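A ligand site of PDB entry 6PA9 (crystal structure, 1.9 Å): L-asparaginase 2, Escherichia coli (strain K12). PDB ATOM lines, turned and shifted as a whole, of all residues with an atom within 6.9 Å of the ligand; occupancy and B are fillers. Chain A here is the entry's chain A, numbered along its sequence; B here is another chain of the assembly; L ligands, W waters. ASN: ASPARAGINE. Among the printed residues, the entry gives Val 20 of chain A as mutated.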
ATOM      1  N   GLY A  18      14.652  -1.059   1.787  1.00  0.00           N
ATOM      2  CA  GLY A  18      14.438   0.380   1.951  1.00  0.00           C
ATOM      3  C   GLY A  18      15.560   1.173   1.273  1.00  0.00           C
ATOM      4  O   GLY A  18      15.933   0.878   0.117  1.00  0.00           O
ATOM      5  N   GLY A  19      16.065   2.228   1.953  1.00  0.00           N
ATOM      6  CA  GLY A  19      17.036   3.105   1.363  1.00  0.00           C
ATOM      7  C   GLY A  19      16.440   4.249   0.539  1.00  0.00           C
ATOM      8  O   GLY A  19      15.238   4.302   0.199  1.00  0.00           O
ATOM      9  N   VAL A  20      17.333   5.204   0.185  1.00  0.00           N
ATOM     10  CA  VAL A  20      16.965   6.236  -0.798  1.00  0.00           C
ATOM     11  C   VAL A  20      16.513   5.688  -2.185  1.00  0.00           C
ATOM     12  O   VAL A  20      15.675   6.322  -2.885  1.00  0.00           O
ATOM     13  CB  VAL A  20      18.111   7.213  -0.985  1.00  0.00           C
ATOM     14  CG1 VAL A  20      17.785   8.246  -2.081  1.00  0.00           C
ATOM     15  CG2 VAL A  20      18.228   7.997   0.325  1.00  0.00           C
ATOM     16  N   ILE A  21      17.074   4.570  -2.569  1.00  0.00           N
ATOM     17  CA  ILE A  21      16.635   3.890  -3.813  1.00  0.00           C
ATOM     18  C   ILE A  21      15.105   3.677  -3.822  1.00  0.00           C
ATOM     19  O   ILE A  21      14.490   3.793  -4.830  1.00  0.00           O
ATOM     20  CB  ILE A  21      17.401   2.599  -4.036  1.00  0.00           C
ATOM     21  CG1 ILE A  21      17.140   2.068  -5.464  1.00  0.00           C
ATOM     22  CG2 ILE A  21      17.111   1.561  -2.913  1.00  0.00           C
ATOM     23  CD1 ILE A  21      18.072   0.942  -5.833  1.00  0.00           C
ATOM     24  N   TYR A  33      16.009  13.992   1.309  1.00  0.00           N
ATOM     25  CA  TYR A  33      15.397  12.770   0.819  1.00  0.00           C
ATOM     26  C   TYR A  33      14.730  11.965   1.999  1.00  0.00           C
ATOM     27  O   TYR A  33      15.184  11.960   3.192  1.00  0.00           O
ATOM     28  CB  TYR A  33      16.464  11.829   0.111  1.00  0.00           C
ATOM     29  CG  TYR A  33      17.380  12.528  -0.916  1.00  0.00           C
ATOM     30  CD1 TYR A  33      16.907  13.591  -1.754  1.00  0.00           C
ATOM     31  CD2 TYR A  33      18.749  12.179  -1.047  1.00  0.00           C
ATOM     32  CE1 TYR A  33      17.747  14.229  -2.721  1.00  0.00           C
ATOM     33  CE2 TYR A  33      19.580  12.779  -2.032  1.00  0.00           C
ATOM     34  CZ  TYR A  33      19.092  13.838  -2.833  1.00  0.00           C
ATOM     35  OH  TYR A  33      19.947  14.478  -3.750  1.00  0.00           O
ATOM     36  N   THR A  34      13.629  11.293   1.618  1.00  0.00           N
ATOM     37  CA  THR A  34      12.977  10.216   2.400  1.00  0.00           C
ATOM     38  C   THR A  34      13.686   8.869   2.105  1.00  0.00           C
ATOM     39  O   THR A  34      14.472   8.708   1.083  1.00  0.00           O
ATOM     40  CB  THR A  34      11.467  10.096   2.063  1.00  0.00           C
ATOM     41  OG1 THR A  34      11.315   9.500   0.747  1.00  0.00           O
ATOM     42  CG2 THR A  34      10.726  11.509   2.124  1.00  0.00           C
ATOM     43  N   VAL A  35      13.476   7.942   3.033  1.00  0.00           N
ATOM     44  CA  VAL A  35      13.974   6.599   2.926  1.00  0.00           C
ATOM     45  C   VAL A  35      12.811   5.598   3.147  1.00  0.00           C
ATOM     46  O   VAL A  35      11.851   5.919   3.868  1.00  0.00           O
ATOM     47  CB  VAL A  35      15.111   6.338   3.953  1.00  0.00           C
ATOM     48  CG1 VAL A  35      16.286   7.230   3.629  1.00  0.00           C
ATOM     49  CG2 VAL A  35      14.636   6.623   5.402  1.00  0.00           C
ATOM     50  N   GLY A  36      12.926   4.442   2.474  1.00  0.00           N
ATOM     51  CA  GLY A  36      11.983   3.281   2.594  1.00  0.00           C
ATOM     52  C   GLY A  36      10.501   3.615   2.474  1.00  0.00           C
ATOM     53  O   GLY A  36       9.694   3.260   3.351  1.00  0.00           O
ATOM     54  N   ILE A  64      13.259   0.588   5.511  1.00  0.00           N
ATOM     55  CA  ILE A  64      13.891   1.541   6.468  1.00  0.00           C
ATOM     56  C   ILE A  64      15.088   2.221   5.830  1.00  0.00           C
ATOM     57  O   ILE A  64      15.649   1.713   4.836  1.00  0.00           O
ATOM     58  CB  ILE A  64      14.375   0.783   7.740  1.00  0.00           C
ATOM     59  CG1 ILE A  64      15.377  -0.348   7.356  1.00  0.00           C
ATOM     60  CG2 ILE A  64      13.175   0.188   8.504  1.00  0.00           C
ATOM     61  CD1 ILE A  64      16.102  -1.026   8.536  1.00  0.00           C
ATOM     62  N   GLY A  65      15.516   3.318   6.473  1.00  0.00           N
ATOM     63  CA  GLY A  65      16.844   3.857   6.175  1.00  0.00           C
ATOM     64  C   GLY A  65      17.906   2.843   6.678  1.00  0.00           C
ATOM     65  O   GLY A  65      17.742   2.251   7.786  1.00  0.00           O
ATOM     66  N   SER A  66      18.937   2.596   5.884  1.00  0.00           N
ATOM     67  CA  SER A  66      19.975   1.643   6.330  1.00  0.00           C
ATOM     68  C   SER A  66      20.821   2.162   7.492  1.00  0.00           C
ATOM     69  O   SER A  66      21.500   1.365   8.092  1.00  0.00           O
ATOM     70  CB  SER A  66      20.852   1.108   5.231  1.00  0.00           C
ATOM     71  OG  SER A  66      21.925   2.053   4.969  1.00  0.00           O
ATOM     72  N   GLN A  67      20.660   3.401   7.894  1.00  0.00           N
ATOM     73  CA  GLN A  67      21.311   3.840   9.111  1.00  0.00           C
ATOM     74  C   GLN A  67      20.648   3.147  10.358  1.00  0.00           C
ATOM     75  O   GLN A  67      21.213   3.168  11.436  1.00  0.00           O
ATOM     76  CB  GLN A  67      21.145   5.358   9.324  1.00  0.00           C
ATOM     77  CG  GLN A  67      19.684   5.968   9.401  1.00  0.00           C
ATOM     78  CD  GLN A  67      19.218   6.486   8.016  1.00  0.00           C
ATOM     79  OE1 GLN A  67      19.350   5.752   6.981  1.00  0.00           O
ATOM     80  NE2 GLN A  67      18.773   7.732   7.973  1.00  0.00           N
ATOM     81  N   ASP A  68      19.435   2.649  10.198  1.00  0.00           N
ATOM     82  CA  ASP A  68      18.767   1.856  11.217  1.00  0.00           C
ATOM     83  C   ASP A  68      18.846   0.326  11.002  1.00  0.00           C
ATOM     84  O   ASP A  68      18.123  -0.442  11.721  1.00  0.00           O
ATOM     85  CB  ASP A  68      17.275   2.255  11.294  1.00  0.00           C
ATOM     86  CG  ASP A  68      17.083   3.684  11.736  1.00  0.00           C
ATOM     87  OD1 ASP A  68      17.962   4.211  12.446  1.00  0.00           O
ATOM     88  OD2 ASP A  68      15.988   4.222  11.475  1.00  0.00           O
ATOM     89  N   HIS A  95      18.770  -1.623  -0.832  1.00  0.00           N
ATOM     90  CA  HIS A  95      19.203  -1.311   0.513  1.00  0.00           C
ATOM     91  C   HIS A  95      19.694   0.142   0.503  1.00  0.00           C
ATOM     92  O   HIS A  95      20.108   0.681  -0.544  1.00  0.00           O
ATOM     93  CB  HIS A  95      20.281  -2.384   0.833  1.00  0.00           C
ATOM     94  CG  HIS A  95      20.760  -2.507   2.284  1.00  0.00           C
ATOM     95  ND1 HIS A  95      21.604  -1.594   2.868  1.00  0.00           N
ATOM     96  CD2 HIS A  95      20.679  -3.552   3.165  1.00  0.00           C
ATOM     97  CE1 HIS A  95      22.005  -2.048   4.050  1.00  0.00           C
ATOM     98  NE2 HIS A  95      21.493  -3.260   4.237  1.00  0.00           N
ATOM     99  N   GLY A  96      19.562   0.790   1.648  1.00  0.00           N
ATOM    100  CA  GLY A  96      20.325   2.012   1.884  1.00  0.00           C
ATOM    101  C   GLY A  96      21.810   1.901   1.628  1.00  0.00           C
ATOM    102  O   GLY A  96      22.462   0.847   1.825  1.00  0.00           O
ATOM    103  N   THR A  97      22.413   3.029   1.253  1.00  0.00           N
ATOM    104  CA  THR A  97      23.858   3.069   1.103  1.00  0.00           C
ATOM    105  C   THR A  97      24.699   3.094   2.398  1.00  0.00           C
ATOM    106  O   THR A  97      25.775   2.521   2.410  1.00  0.00           O
ATOM    107  CB  THR A  97      24.313   4.259   0.233  1.00  0.00           C
ATOM    108  OG1 THR A  97      23.799   5.442   0.772  1.00  0.00           O
ATOM    109  CG2 THR A  97      23.807   4.037  -1.197  1.00  0.00           C
ATOM    110  N   ASP A  98      24.167   3.714   3.447  1.00  0.00           N
ATOM    111  CA  ASP A  98      24.943   3.978   4.664  1.00  0.00           C
ATOM    112  C   ASP A  98      25.606   2.755   5.280  1.00  0.00           C
ATOM    113  O   ASP A  98      26.788   2.801   5.654  1.00  0.00           O
ATOM    114  CB  ASP A  98      24.085   4.725   5.683  1.00  0.00           C
ATOM    115  CG  ASP A  98      23.597   6.034   5.208  1.00  0.00           C
ATOM    116  OD1 ASP A  98      24.018   6.507   4.114  1.00  0.00           O
ATOM    117  OD2 ASP A  98      22.771   6.627   5.912  1.00  0.00           O
ATOM    118  N   THR A  99      24.861   1.657   5.387  1.00  0.00           N
ATOM    119  CA  THR A  99      25.376   0.404   5.953  1.00  0.00           C
ATOM    120  C   THR A  99      25.334  -0.786   4.968  1.00  0.00           C
ATOM    121  O   THR A  99      25.512  -1.916   5.392  1.00  0.00           O
ATOM    122  CB  THR A  99      24.645   0.035   7.248  1.00  0.00           C
ATOM    123  OG1 THR A  99      23.248  -0.243   6.951  1.00  0.00           O
ATOM    124  CG2 THR A  99      24.763   1.257   8.245  1.00  0.00           C
ATOM    125  N   MET A 100      25.152  -0.502   3.683  1.00  0.00           N
ATOM    126  CA  MET A 100      25.282  -1.507   2.632  1.00  0.00           C
ATOM    127  C   MET A 100      26.495  -2.426   2.772  1.00  0.00           C
ATOM    128  O   MET A 100      26.410  -3.651   2.597  1.00  0.00           O
ATOM    129  CB  MET A 100      25.251  -0.870   1.257  1.00  0.00           C
ATOM    130  CG  MET A 100      25.256  -1.958   0.160  1.00  0.00           C
ATOM    131  SD  MET A 100      24.311  -1.676  -1.308  1.00  0.00           S
ATOM    132  CE  MET A 100      25.097  -0.153  -1.810  1.00  0.00           C
ATOM    133  N   GLY A 121      22.026   0.098  -4.119  1.00  0.00           N
ATOM    134  CA  GLY A 121      21.427   1.295  -3.547  1.00  0.00           C
ATOM    135  C   GLY A 121      21.444   2.462  -4.528  1.00  0.00           C
ATOM    136  O   GLY A 121      21.769   2.306  -5.699  1.00  0.00           O
ATOM    137  N   ALA A 122      21.027   3.624  -4.050  1.00  0.00           N
ATOM    138  CA  ALA A 122      21.127   4.836  -4.831  1.00  0.00           C
ATOM    139  C   ALA A 122      21.552   5.986  -3.904  1.00  0.00           C
ATOM    140  O   ALA A 122      21.004   6.104  -2.813  1.00  0.00           O
ATOM    141  CB  ALA A 122      19.775   5.192  -5.426  1.00  0.00           C
ATOM    142  N   MET A 123      22.352   6.879  -4.407  1.00  0.00           N
ATOM    143  CA  MET A 123      22.744   8.113  -3.701  1.00  0.00           C
ATOM    144  C   MET A 123      21.775   9.280  -3.904  1.00  0.00           C
ATOM    145  O   MET A 123      21.703  10.174  -3.047  1.00  0.00           O
ATOM    146  CB  MET A 123      24.166   8.544  -4.091  1.00  0.00           C
ATOM    147  CG  MET A 123      25.203   7.542  -3.661  1.00  0.00           C
ATOM    148  SD  MET A 123      25.382   7.317  -1.918  1.00  0.00           S
ATOM    149  CE  MET A 123      26.270   8.827  -1.582  1.00  0.00           C
ATOM    150  N   ARG A 124      20.942   9.239  -4.938  1.00  0.00           N
ATOM    151  CA  ARG A 124      19.922  10.241  -5.156  1.00  0.00           C
ATOM    152  C   ARG A 124      18.542   9.530  -5.273  1.00  0.00           C
ATOM    153  O   ARG A 124      18.457   8.437  -5.823  1.00  0.00           O
ATOM    154  CB  ARG A 124      20.261  11.019  -6.425  1.00  0.00           C
ATOM    155  CG  ARG A 124      21.644  11.663  -6.486  1.00  0.00           C
ATOM    156  CD  ARG A 124      22.050  12.064  -7.938  1.00  0.00           C
ATOM    157  NE  ARG A 124      23.367  12.720  -8.046  1.00  0.00           N
ATOM    158  CZ  ARG A 124      24.093  12.810  -9.154  1.00  0.00           C
ATOM    159  NH1 ARG A 124      23.628  12.301 -10.294  1.00  0.00           N
ATOM    160  NH2 ARG A 124      25.320  13.411  -9.162  1.00  0.00           N
ATOM    161  N   LYS A 170      31.891   2.473   1.558  1.00  0.00           N
ATOM    162  CA  LYS A 170      31.379   3.770   1.115  1.00  0.00           C
ATOM    163  C   LYS A 170      32.445   4.795   1.387  1.00  0.00           C
ATOM    164  O   LYS A 170      32.740   5.056   2.533  1.00  0.00           O
ATOM    165  CB  LYS A 170      30.055   4.077   1.821  1.00  0.00           C
ATOM    166  CG  LYS A 170      29.357   5.341   1.313  1.00  0.00           C
ATOM    167  CD  LYS A 170      27.966   5.545   1.929  1.00  0.00           C
ATOM    168  CE  LYS A 170      27.302   6.819   1.392  1.00  0.00           C
ATOM    169  NZ  LYS A 170      25.890   6.877   1.834  1.00  0.00           N
ATOM    170  N   VAL B 252      26.993   7.348   9.784  1.00  0.00           N
ATOM    171  CA  VAL B 252      27.064   6.537   8.621  1.00  0.00           C
ATOM    172  C   VAL B 252      26.620   7.417   7.463  1.00  0.00           C
ATOM    173  O   VAL B 252      25.707   8.300   7.600  1.00  0.00           O
ATOM    174  CB  VAL B 252      26.219   5.282   8.759  1.00  0.00           C
ATOM    175  CG1 VAL B 252      26.815   4.389   9.824  1.00  0.00           C
ATOM    176  CG2 VAL B 252      24.759   5.587   9.141  1.00  0.00           C
ATOM    177  N   GLY B 253      27.225   7.174   6.286  1.00  0.00           N
ATOM    178  CA  GLY B 253      26.877   7.987   5.106  1.00  0.00           C
ATOM    179  C   GLY B 253      27.072   9.482   5.382  1.00  0.00           C
ATOM    180  O   GLY B 253      28.053   9.889   6.003  1.00  0.00           O
ATOM    181  N   ASN B 254      26.084  10.284   4.973  1.00  0.00           N
ATOM    182  CA  ASN B 254      26.098  11.734   5.110  1.00  0.00           C
ATOM    183  C   ASN B 254      25.675  12.079   6.531  1.00  0.00           C
ATOM    184  O   ASN B 254      24.629  12.729   6.754  1.00  0.00           O
ATOM    185  CB  ASN B 254      25.156  12.342   4.075  1.00  0.00           C
ATOM    186  CG  ASN B 254      25.302  13.862   3.978  1.00  0.00           C
ATOM    187  OD1 ASN B 254      26.084  14.478   4.779  1.00  0.00           O
ATOM    188  ND2 ASN B 254      24.685  14.470   2.942  1.00  0.00           N
ATOM    189  N   ASN B 256      24.560  10.348   9.096  1.00  0.00           N
ATOM    190  CA  ASN B 256      23.326   9.825   9.724  1.00  0.00           C
ATOM    191  C   ASN B 256      23.641   9.042  11.002  1.00  0.00           C
ATOM    192  O   ASN B 256      24.762   8.587  11.227  1.00  0.00           O
ATOM    193  CB  ASN B 256      22.520   8.995   8.731  1.00  0.00           C
ATOM    194  CG  ASN B 256      21.927   9.835   7.608  1.00  0.00           C
ATOM    195  OD1 ASN B 256      21.337  10.888   7.899  1.00  0.00           O
ATOM    196  ND2 ASN B 256      22.185   9.442   6.290  1.00  0.00           N
ATOM    197  N   GLU B 291      19.229  14.314   5.330  1.00  0.00           N
ATOM    198  CA  GLU B 291      18.157  13.582   6.045  1.00  0.00           C
ATOM    199  C   GLU B 291      17.861  14.131   7.439  1.00  0.00           C
ATOM    200  O   GLU B 291      16.869  13.753   8.025  1.00  0.00           O
ATOM    201  CB  GLU B 291      18.430  12.074   6.124  1.00  0.00           C
ATOM    202  CG  GLU B 291      18.315  11.379   4.759  1.00  0.00           C
ATOM    203  CD  GLU B 291      18.814   9.938   4.782  1.00  0.00           C
ATOM    204  OE1 GLU B 291      18.178   9.213   5.573  1.00  0.00           O
ATOM    205  OE2 GLU B 291      19.895   9.625   4.142  1.00  0.00           O
HETATM  206  N   ASN L   1      20.387   7.083   4.660  1.00  0.00           N
HETATM  207  CA  ASN L   1      20.173   6.408   3.365  1.00  0.00           C
HETATM  208  C   ASN L   1      20.189   4.928   3.648  1.00  0.00           C
HETATM  209  O   ASN L   1      19.120   4.275   3.703  1.00  0.00           O
HETATM  210  CB  ASN L   1      21.258   6.806   2.343  1.00  0.00           C
HETATM  211  CG  ASN L   1      20.964   6.298   0.925  1.00  0.00           C
HETATM  212  OD1 ASN L   1      20.435   5.208   0.750  1.00  0.00           O
HETATM  213  ND2 ASN L   1      21.379   7.075  -0.088  1.00  0.00           N
HETATM  214  OXT ASN L   1      21.265   4.400   3.848  1.00  0.00           O
HETATM  215  O   HOH W   1      22.066   9.837  -0.238  1.00  0.00           O
HETATM  216  O   HOH W   2      19.747   3.423  -1.357  1.00  0.00           O
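OE2 of Glu 291 of chain B lies within salt-bridge range of N of the ligand, at 2.6 Å.
The backbone NH of Ser 66 sits at hydrogen-bond distance from an oxygen (O) of the ligand, 2.8 Å away.
The side-chain hydroxyl of Ser 66 lies within hydrogen-bond range of an oxygen (OXT) of the ligand (2.7 Å).
N of Asp 98 sits at hydrogen-bond distance from OXT of the ligand.
A nitrogen (N) of the ligand lies within salt-bridge range of the side-chain carboxylate of Asp 98 (2.7 Å).
The side-chain amide oxygen (OE1) of Gln 67 lies within hydrogen-bond range of a nitrogen (N) of the ligand (2.9 Å).
O of Ala 122 lies within hydrogen-bond range of ND2 of the ligand (2.9 Å).
OD1 of the ligand sits at hydrogen-bond distance from N of Thr 97 (3.0 Å).
OG1 of Thr 97 sits close to ND2 of the ligand (3.0 Å).
OD1 of the ligand lies within hydrogen-bond range of N of Val 20 (3.2 Å).
N of the ligand lies close to ND2 of Asn 256 of chain B (3.4 Å).
The side-chain amide nitrogen (NE2) of Gln 67 is in hydrogen-bond range of the side-chain carboxylate (OE1) of Glu 291 of chain B (2.9 Å).
OE2 of Glu 291 of chain B sits at hydrogen-bond distance from ND2 of Asn 256 of chain B (3.1 Å).
The side-chain hydroxyl (OG) of Ser 66 sits at hydrogen-bond distance from the backbone NH (N) of Asp 98 (3.2 Å).
The side-chain hydroxyl (OG) of Ser 66 sits close to the backbone carbonyl oxygen (O) of Gly 96 (3.4 Å).
The backbone carbonyl oxygen (O) of Ser 66 is in hydrogen-bond range of the side-chain hydroxyl (OG1) of Thr 99, at 2.6 Å.
OD2 of Asp 98 is in hydrogen-bond range of ND2 of Asn 256 of chain B.
The side-chain carboxylate of Asp 98 is in salt-bridge range of the side-chain amino group of Lys 170 (3.0 Å).
OG1 of Thr 97 sits at hydrogen-bond distance from NZ of Lys 170, at 2.7 Å.
Water W1 bridges a nitrogen (ND2) of the ligand (2.9 Å) and the backbone carbonyl oxygen of Met 123 (2.9 Å).
Gly 19 touches the ligand.
Val 35 touches the ligand (CG1 to CA, 3.98 Å).
CA of Gly 65 touches O of the ligand, 3.4 Å away.
Gly 96 touches the ligand (CA to O, 3.1 Å).
CA of Met 123 touches ND2 of the ligand, at 3.999 Å.
Hydrophobic or aromatic side chains that line the ligand: Val 20 and Val 35.
13 residues have an atom within 4 Å of the ligand: Gly 19, Val 20, Val 35, Gly 65, Ser 66, Gln 67, Gly 96, Thr 97, Asp 98, Ala 122, Met 123, Asn 256 of chain B and Glu 291 of chain B.
The nearest printed residue that does not touch the ligand is Ile 64 (4.5 Å).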
